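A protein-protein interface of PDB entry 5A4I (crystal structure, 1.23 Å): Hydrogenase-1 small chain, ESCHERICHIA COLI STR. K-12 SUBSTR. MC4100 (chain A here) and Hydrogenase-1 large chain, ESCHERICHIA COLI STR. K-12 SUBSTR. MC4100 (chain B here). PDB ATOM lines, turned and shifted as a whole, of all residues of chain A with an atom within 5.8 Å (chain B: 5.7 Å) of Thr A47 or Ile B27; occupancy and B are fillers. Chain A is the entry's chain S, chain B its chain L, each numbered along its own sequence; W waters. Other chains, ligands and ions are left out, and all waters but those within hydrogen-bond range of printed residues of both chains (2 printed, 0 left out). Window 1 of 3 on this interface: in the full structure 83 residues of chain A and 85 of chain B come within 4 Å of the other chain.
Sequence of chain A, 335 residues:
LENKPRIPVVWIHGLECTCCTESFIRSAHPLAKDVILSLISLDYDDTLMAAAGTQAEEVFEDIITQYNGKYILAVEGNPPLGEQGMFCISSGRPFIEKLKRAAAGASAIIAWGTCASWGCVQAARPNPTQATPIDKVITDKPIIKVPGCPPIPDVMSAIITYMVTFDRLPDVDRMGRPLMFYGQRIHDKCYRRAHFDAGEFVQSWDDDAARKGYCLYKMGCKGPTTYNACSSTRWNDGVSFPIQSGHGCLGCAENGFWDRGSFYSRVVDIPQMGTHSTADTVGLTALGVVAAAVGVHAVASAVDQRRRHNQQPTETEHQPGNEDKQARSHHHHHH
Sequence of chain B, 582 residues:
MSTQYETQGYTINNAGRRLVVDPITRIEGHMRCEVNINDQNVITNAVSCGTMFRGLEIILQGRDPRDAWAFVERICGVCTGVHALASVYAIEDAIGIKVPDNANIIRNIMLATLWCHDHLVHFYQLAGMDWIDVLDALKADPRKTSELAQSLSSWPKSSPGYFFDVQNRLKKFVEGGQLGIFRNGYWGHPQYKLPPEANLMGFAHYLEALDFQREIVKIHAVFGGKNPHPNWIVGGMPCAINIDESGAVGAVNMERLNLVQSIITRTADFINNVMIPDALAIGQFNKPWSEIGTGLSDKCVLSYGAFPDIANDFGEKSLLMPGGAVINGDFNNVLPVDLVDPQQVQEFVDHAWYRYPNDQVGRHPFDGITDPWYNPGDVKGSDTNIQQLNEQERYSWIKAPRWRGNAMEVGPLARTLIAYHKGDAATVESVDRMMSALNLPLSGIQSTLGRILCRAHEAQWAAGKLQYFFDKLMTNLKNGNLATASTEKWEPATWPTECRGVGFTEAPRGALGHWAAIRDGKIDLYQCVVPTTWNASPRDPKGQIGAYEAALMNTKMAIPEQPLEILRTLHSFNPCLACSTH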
ATOM      1  N   HIS A  13      -2.693 -24.599 -11.271  1.00  0.00           N
ATOM      2  CA  HIS A  13      -1.769 -24.151 -12.302  1.00  0.00           C
ATOM      3  C   HIS A  13      -0.660 -23.335 -11.676  1.00  0.00           C
ATOM      4  O   HIS A  13      -0.911 -22.292 -11.091  1.00  0.00           O
ATOM      5  CB  HIS A  13      -2.510 -23.252 -13.339  1.00  0.00           C
ATOM      6  CG  HIS A  13      -3.619 -23.922 -14.064  1.00  0.00           C
ATOM      7  ND1 HIS A  13      -3.469 -24.435 -15.323  1.00  0.00           N
ATOM      8  CD2 HIS A  13      -4.892 -24.179 -13.708  1.00  0.00           C
ATOM      9  CE1 HIS A  13      -4.623 -24.912 -15.747  1.00  0.00           C
ATOM     10  NE2 HIS A  13      -5.496 -24.800 -14.759  1.00  0.00           N
ATOM     11  N   THR A  18      -0.007 -23.544 -20.285  1.00  0.00           N
ATOM     12  CA  THR A  18      -1.388 -23.971 -20.437  1.00  0.00           C
ATOM     13  C   THR A  18      -1.606 -24.970 -21.557  1.00  0.00           C
ATOM     14  O   THR A  18      -2.748 -25.348 -21.872  1.00  0.00           O
ATOM     15  CB  THR A  18      -2.329 -22.781 -20.431  1.00  0.00           C
ATOM     16  OG1 THR A  18      -1.965 -21.894 -19.350  1.00  0.00           O
ATOM     17  CG2 THR A  18      -3.790 -23.150 -20.221  1.00  0.00           C
ATOM     18  N   THR A  21      -3.701 -28.133 -20.407  1.00  0.00           N
ATOM     19  CA  THR A  21      -5.139 -27.912 -20.361  1.00  0.00           C
ATOM     20  C   THR A  21      -5.709 -27.917 -21.779  1.00  0.00           C
ATOM     21  O   THR A  21      -6.772 -28.481 -22.031  1.00  0.00           O
ATOM     22  CB  THR A  21      -5.442 -26.569 -19.667  1.00  0.00           C
ATOM     23  OG1 THR A  21      -5.330 -26.723 -18.265  1.00  0.00           O
ATOM     24  CG2 THR A  21      -6.851 -26.057 -19.969  1.00  0.00           C
ATOM     25  N   ASP A  45     -10.778 -25.045 -11.320  1.00  0.00           N
ATOM     26  CA  ASP A  45      -9.902 -24.978 -12.467  1.00  0.00           C
ATOM     27  C   ASP A  45      -9.887 -23.514 -12.957  1.00  0.00           C
ATOM     28  O   ASP A  45     -10.858 -23.055 -13.521  1.00  0.00           O
ATOM     29  CB  ASP A  45     -10.353 -25.901 -13.594  1.00  0.00           C
ATOM     30  CG  ASP A  45      -9.322 -26.002 -14.694  1.00  0.00           C
ATOM     31  OD1 ASP A  45      -8.447 -25.097 -14.795  1.00  0.00           O
ATOM     32  OD2 ASP A  45      -9.327 -27.042 -15.370  1.00  0.00           O
ATOM     33  N   ASP A  46      -8.780 -22.814 -12.790  1.00  0.00           N
ATOM     34  CA  ASP A  46      -8.761 -21.385 -13.108  1.00  0.00           C
ATOM     35  C   ASP A  46      -9.071 -21.087 -14.573  1.00  0.00           C
ATOM     36  O   ASP A  46      -9.631 -20.036 -14.848  1.00  0.00           O
ATOM     37  CB  ASP A  46      -7.455 -20.699 -12.699  1.00  0.00           C
ATOM     38  CG  ASP A  46      -7.349 -20.407 -11.137  1.00  0.00           C
ATOM     39  OD1 ASP A  46      -8.343 -20.530 -10.343  1.00  0.00           O
ATOM     40  OD2 ASP A  46      -6.260 -20.007 -10.694  1.00  0.00           O
ATOM     41  N   THR A  47      -8.739 -21.979 -15.491  1.00  0.00           N
ATOM     42  CA  THR A  47      -8.921 -21.704 -16.903  1.00  0.00           C
ATOM     43  C   THR A  47     -10.388 -21.701 -17.314  1.00  0.00           C
ATOM     44  O   THR A  47     -10.774 -20.968 -18.245  1.00  0.00           O
ATOM     45  CB  THR A  47      -8.164 -22.731 -17.788  1.00  0.00           C
ATOM     46  OG1 THR A  47      -6.891 -22.987 -17.233  1.00  0.00           O
ATOM     47  CG2 THR A  47      -7.978 -22.174 -19.159  1.00  0.00           C
ATOM     48  N   LEU A  48     -11.228 -22.501 -16.652  1.00  0.00           N
ATOM     49  CA  LEU A  48     -12.583 -22.778 -17.148  1.00  0.00           C
ATOM     50  C   LEU A  48     -13.691 -22.324 -16.196  1.00  0.00           C
ATOM     51  O   LEU A  48     -14.840 -22.228 -16.612  1.00  0.00           O
ATOM     52  CB  LEU A  48     -12.779 -24.255 -17.448  1.00  0.00           C
ATOM     53  CG  LEU A  48     -11.895 -24.835 -18.537  1.00  0.00           C
ATOM     54  CD1 LEU A  48     -12.127 -26.330 -18.620  1.00  0.00           C
ATOM     55  CD2 LEU A  48     -12.183 -24.153 -19.870  1.00  0.00           C
ATOM     56  N   MET A  49     -13.363 -22.062 -14.941  1.00  0.00           N
ATOM     57  CA  MET A  49     -14.422 -21.877 -13.946  1.00  0.00           C
ATOM     58  C   MET A  49     -15.093 -20.474 -14.038  1.00  0.00           C
ATOM     59  O   MET A  49     -14.468 -19.469 -14.383  1.00  0.00           O
ATOM     60  CB  MET A  49     -13.862 -22.144 -12.541  1.00  0.00           C
ATOM     61  CG  MET A  49     -12.867 -21.151 -12.012  1.00  0.00           C
ATOM     62  SD  MET A  49     -11.978 -21.751 -10.546  1.00  0.00           S
ATOM     63  CE  MET A  49     -13.270 -21.625  -9.340  1.00  0.00           C
ATOM     64  N   ILE B  24      -7.740 -13.812 -11.320  1.00  0.00           N
ATOM     65  CA  ILE B  24      -8.634 -13.674 -12.469  1.00  0.00           C
ATOM     66  C   ILE B  24      -8.698 -15.058 -13.122  1.00  0.00           C
ATOM     67  O   ILE B  24      -7.687 -15.686 -13.371  1.00  0.00           O
ATOM     68  CB  ILE B  24      -8.119 -12.630 -13.473  1.00  0.00           C
ATOM     69  CG1 ILE B  24      -7.947 -11.210 -12.828  1.00  0.00           C
ATOM     70  CG2 ILE B  24      -8.987 -12.620 -14.724  1.00  0.00           C
ATOM     71  CD1 ILE B  24      -9.245 -10.542 -12.518  1.00  0.00           C
ATOM     72  N   THR B  25      -9.884 -15.567 -13.339  1.00  0.00           N
ATOM     73  CA  THR B  25     -10.104 -16.869 -13.962  1.00  0.00           C
ATOM     74  C   THR B  25     -10.651 -16.690 -15.377  1.00  0.00           C
ATOM     75  O   THR B  25     -10.954 -15.574 -15.794  1.00  0.00           O
ATOM     76  CB  THR B  25     -11.046 -17.701 -13.100  1.00  0.00           C
ATOM     77  OG1 THR B  25     -12.252 -16.949 -12.935  1.00  0.00           O
ATOM     78  CG2 THR B  25     -10.416 -18.033 -11.731  1.00  0.00           C
ATOM     79  N   ARG B  26     -10.761 -17.803 -16.098  1.00  0.00           N
ATOM     80  CA  ARG B  26     -11.167 -17.779 -17.516  1.00  0.00           C
ATOM     81  C   ARG B  26     -10.286 -16.877 -18.339  1.00  0.00           C
ATOM     82  O   ARG B  26     -10.743 -16.144 -19.233  1.00  0.00           O
ATOM     83  CB  ARG B  26     -12.675 -17.564 -17.679  1.00  0.00           C
ATOM     84  CG  ARG B  26     -13.448 -18.855 -17.434  1.00  0.00           C
ATOM     85  CD  ARG B  26     -14.936 -18.700 -17.512  1.00  0.00           C
ATOM     86  NE  ARG B  26     -15.480 -17.790 -16.517  1.00  0.00           N
ATOM     87  CZ  ARG B  26     -16.173 -16.670 -16.768  1.00  0.00           C
ATOM     88  NH1 ARG B  26     -16.369 -16.179 -17.957  1.00  0.00           N
ATOM     89  NH2 ARG B  26     -16.696 -16.009 -15.726  1.00  0.00           N
ATOM     90  N   ILE B  27      -9.000 -16.962 -18.018  1.00  0.00           N
ATOM     91  CA  ILE B  27      -7.902 -16.393 -18.793  1.00  0.00           C
ATOM     92  C   ILE B  27      -6.853 -17.482 -18.884  1.00  0.00           C
ATOM     93  O   ILE B  27      -6.910 -18.489 -18.163  1.00  0.00           O
ATOM     94  CB  ILE B  27      -7.311 -15.125 -18.170  1.00  0.00           C
ATOM     95  CG1 ILE B  27      -6.747 -15.393 -16.774  1.00  0.00           C
ATOM     96  CG2 ILE B  27      -8.347 -14.033 -18.130  1.00  0.00           C
ATOM     97  CD1 ILE B  27      -5.852 -14.329 -16.200  1.00  0.00           C
ATOM     98  N   GLU B  28      -5.831 -17.249 -19.701  1.00  0.00           N
ATOM     99  CA  GLU B  28      -4.617 -18.056 -19.569  1.00  0.00           C
ATOM    100  C   GLU B  28      -3.707 -17.405 -18.514  1.00  0.00           C
ATOM    101  O   GLU B  28      -3.501 -16.177 -18.521  1.00  0.00           O
ATOM    102  CB  GLU B  28      -3.893 -18.150 -20.898  1.00  0.00           C
ATOM    103  CG  GLU B  28      -2.731 -19.120 -20.875  1.00  0.00           C
ATOM    104  CD  GLU B  28      -1.560 -18.727 -20.030  1.00  0.00           C
ATOM    105  OE1 GLU B  28      -1.305 -17.511 -19.920  1.00  0.00           O
ATOM    106  OE2 GLU B  28      -0.840 -19.605 -19.476  1.00  0.00           O
ATOM    107  N   GLY B  29      -3.184 -18.198 -17.602  1.00  0.00           N
ATOM    108  CA  GLY B  29      -2.122 -17.751 -16.708  1.00  0.00           C
ATOM    109  C   GLY B  29      -2.621 -16.969 -15.533  1.00  0.00           C
ATOM    110  O   GLY B  29      -3.769 -17.109 -15.115  1.00  0.00           O
ATOM    111  N   HIS B  30      -1.722 -16.207 -14.950  1.00  0.00           N
ATOM    112  CA  HIS B  30      -1.894 -15.613 -13.616  1.00  0.00           C
ATOM    113  C   HIS B  30      -1.986 -14.104 -13.696  1.00  0.00           C
ATOM    114  O   HIS B  30      -1.038 -13.444 -14.124  1.00  0.00           O
ATOM    115  CB  HIS B  30      -0.688 -16.017 -12.747  1.00  0.00           C
ATOM    116  CG  HIS B  30      -0.615 -17.494 -12.526  1.00  0.00           C
ATOM    117  ND1 HIS B  30      -1.411 -18.108 -11.610  1.00  0.00           N
ATOM    118  CD2 HIS B  30       0.114 -18.466 -13.101  1.00  0.00           C
ATOM    119  CE1 HIS B  30      -1.143 -19.392 -11.572  1.00  0.00           C
ATOM    120  NE2 HIS B  30      -0.248 -19.639 -12.498  1.00  0.00           N
ATOM    121  N   MET B  31      -3.149 -13.589 -13.274  1.00  0.00           N
ATOM    122  CA  MET B  31      -3.376 -12.165 -13.228  1.00  0.00           C
ATOM    123  C   MET B  31      -4.081 -11.805 -11.928  1.00  0.00           C
ATOM    124  O   MET B  31      -4.940 -12.530 -11.433  1.00  0.00           O
ATOM    125  CB  MET B  31      -4.273 -11.674 -14.377  1.00  0.00           C
ATOM    126  CG  MET B  31      -4.383 -10.166 -14.494  1.00  0.00           C
ATOM    127  SD  MET B  31      -5.442  -9.677 -15.863  1.00  0.00           S
ATOM    128  CE  MET B  31      -5.561  -7.932 -15.481  1.00  0.00           C
ATOM    129  N   GLN B 125     -15.705 -20.699 -24.157  1.00  0.00           N
ATOM    130  CA  GLN B 125     -15.171 -21.241 -22.924  1.00  0.00           C
ATOM    131  C   GLN B 125     -14.602 -20.175 -21.986  1.00  0.00           C
ATOM    132  O   GLN B 125     -14.615 -20.387 -20.764  1.00  0.00           O
ATOM    133  CB  GLN B 125     -14.101 -22.290 -23.206  1.00  0.00           C
ATOM    134  CG  GLN B 125     -14.656 -23.678 -23.455  1.00  0.00           C
ATOM    135  CD  GLN B 125     -15.505 -23.737 -24.710  1.00  0.00           C
ATOM    136  OE1 GLN B 125     -15.030 -23.438 -25.819  1.00  0.00           O
ATOM    137  NE2 GLN B 125     -16.771 -24.121 -24.546  1.00  0.00           N
ATOM    138  N   LEU B 126     -14.126 -19.047 -22.523  1.00  0.00           N
ATOM    139  CA  LEU B 126     -13.487 -18.042 -21.673  1.00  0.00           C
ATOM    140  C   LEU B 126     -14.432 -16.890 -21.362  1.00  0.00           C
ATOM    141  O   LEU B 126     -14.748 -16.623 -20.196  1.00  0.00           O
ATOM    142  CB  LEU B 126     -12.144 -17.619 -22.254  1.00  0.00           C
ATOM    143  CG  LEU B 126     -11.126 -18.748 -22.462  1.00  0.00           C
ATOM    144  CD1 LEU B 126      -9.831 -18.247 -23.077  1.00  0.00           C
ATOM    145  CD2 LEU B 126     -10.894 -19.546 -21.186  1.00  0.00           C
ATOM    146  N   HIS B 571     -12.050  -9.896 -19.886  1.00  0.00           N
ATOM    147  CA  HIS B 571     -12.162 -11.033 -20.783  1.00  0.00           C
ATOM    148  C   HIS B 571     -12.344 -10.597 -22.222  1.00  0.00           C
ATOM    149  O   HIS B 571     -11.940 -11.330 -23.138  1.00  0.00           O
ATOM    150  CB  HIS B 571     -13.319 -11.935 -20.394  1.00  0.00           C
ATOM    151  CG  HIS B 571     -13.104 -12.726 -19.150  1.00  0.00           C
ATOM    152  ND1 HIS B 571     -14.137 -13.078 -18.335  1.00  0.00           N
ATOM    153  CD2 HIS B 571     -11.996 -13.267 -18.590  1.00  0.00           C
ATOM    154  CE1 HIS B 571     -13.688 -13.807 -17.328  1.00  0.00           C
ATOM    155  NE2 HIS B 571     -12.393 -13.932 -17.462  1.00  0.00           N
ATOM    156  N   PRO B 575      -7.148 -12.017 -22.218  1.00  0.00           N
ATOM    157  CA  PRO B 575      -5.802 -11.927 -21.595  1.00  0.00           C
ATOM    158  C   PRO B 575      -5.059 -13.261 -21.647  1.00  0.00           C
ATOM    159  O   PRO B 575      -5.595 -14.315 -21.253  1.00  0.00           O
ATOM    160  CB  PRO B 575      -6.113 -11.539 -20.145  1.00  0.00           C
ATOM    161  CG  PRO B 575      -7.471 -10.875 -20.195  1.00  0.00           C
ATOM    162  CD  PRO B 575      -8.197 -11.672 -21.232  1.00  0.00           C
ATOM    163  N   CYS B 576      -3.774 -13.175 -22.022  1.00  0.00           N
ATOM    164  CA  CYS B 576      -2.890 -14.336 -21.937  1.00  0.00           C
ATOM    165  C   CYS B 576      -1.683 -13.907 -21.124  1.00  0.00           C
ATOM    166  O   CYS B 576      -0.787 -13.170 -21.607  1.00  0.00           O
ATOM    167  CB  CYS B 576      -2.462 -14.753 -23.319  1.00  0.00           C
ATOM    168  SG  CYS B 576      -1.600 -16.331 -23.183  1.00  0.00           S
ATOM    169  N   LEU B 577      -1.644 -14.329 -19.876  1.00  0.00           N
ATOM    170  CA  LEU B 577      -0.637 -13.804 -18.967  1.00  0.00           C
ATOM    171  C   LEU B 577       0.705 -14.464 -19.127  1.00  0.00           C
ATOM    172  O   LEU B 577       1.722 -13.802 -18.919  1.00  0.00           O
ATOM    173  CB  LEU B 577      -1.147 -13.874 -17.550  1.00  0.00           C
ATOM    174  CG  LEU B 577      -2.050 -12.700 -17.165  1.00  0.00           C
ATOM    175  CD1 LEU B 577      -1.262 -11.436 -16.957  1.00  0.00           C
ATOM    176  CD2 LEU B 577      -3.201 -12.438 -18.115  1.00  0.00           C
HETATM  177  O   HOH W   1      -3.539 -20.951 -17.135  1.00  0.00           O
HETATM  178  O   HOH W   2     -15.586 -22.475 -19.297  1.00  0.00           O
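The backbone NH (N) of Asp A45 sits at hydrogen-bond distance from the side-chain sulfur (SD) of Met A49, 3.6 Å away.
A ring nitrogen (NE2) of His A13 is in hydrogen-bond range of the side-chain carboxylate (OD1) of Asp A45 (3.0 Å).
N of Thr A47 lies close to OD1 of Asp A45, 3.2 Å away.
O of Pro B575 is in hydrogen-bond range of N of Glu B28, 3.3 Å away.
NE2 of His A13 lies close to OG1 of Thr A47.
O of Glu B28 lies within hydrogen-bond range of N of Leu B577, 2.9 Å away.
Thr A47 touches just these residues of chain B: Arg B26 (3.3 Å), Ile B27 (3.96 Å) and Leu B126 (3.3 Å).
Of chain A, only Thr A47 (3.96 Å) comes within 4 Å of Ile B27.
Printed residues of chain A within 4 Å of Leu B126: Thr A47 (3.3 Å).
Printed residues of chain A within 4 Å of Glu B28: Thr A18 (2.6 Å).
Of the printed residues of chain B, Leu A48 touches Arg B26 (3.6 Å).
Printed residues of chain B within 4 Å of His A13: His B30 (2.9 Å).
Printed residues of chain B within 4 Å of Met A49: Thr B25 (3.7 Å) and Arg B26 (2.9 Å).
Gln B125 touches none of the printed residues of chain A.
Leu B577 touches none of the printed residues of chain A.
The nearest printed residue of chain A that does not touch His B30 is Asp A46 (5.2 Å).
OE2 of Glu B28 lies within hydrogen-bond range of OG1 of Thr A18, 2.6 Å away.
The backbone carbonyl oxygen (O) of Asp A46 sits at hydrogen-bond distance from the backbone NH (N) of Arg B26, at 2.8 Å.
O of Met A49 lies within hydrogen-bond range of NE of Arg B26, at 2.9 Å.
The backbone carbonyl oxygen (O) of His A13 sits close to a ring nitrogen (NE2) of His B30.
Among the printed residues, pairs that only touch across the chains: Asp A46 with Thr B25, Thr A47 with Arg B26, Thr A47 with Ile B27, Thr A47 with Leu B126, Leu A48 with Arg B26 and Met A49 with Thr B25.
Of the 14 printed residues of chain B, 6 touch a printed residue of chain A.
Of the 8 printed residues of chain A, 6 touch a printed residue of chain B.
Among the printed residues, no Asp or Glu carboxylate lies within 4 Å of a Lys or Arg side-chain nitrogen of the other chain.
Water W2 bridges O of Gln B125 and O of Leu A48.
Water W1 bridges N of Gly B29 and OG1 of Thr A18.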
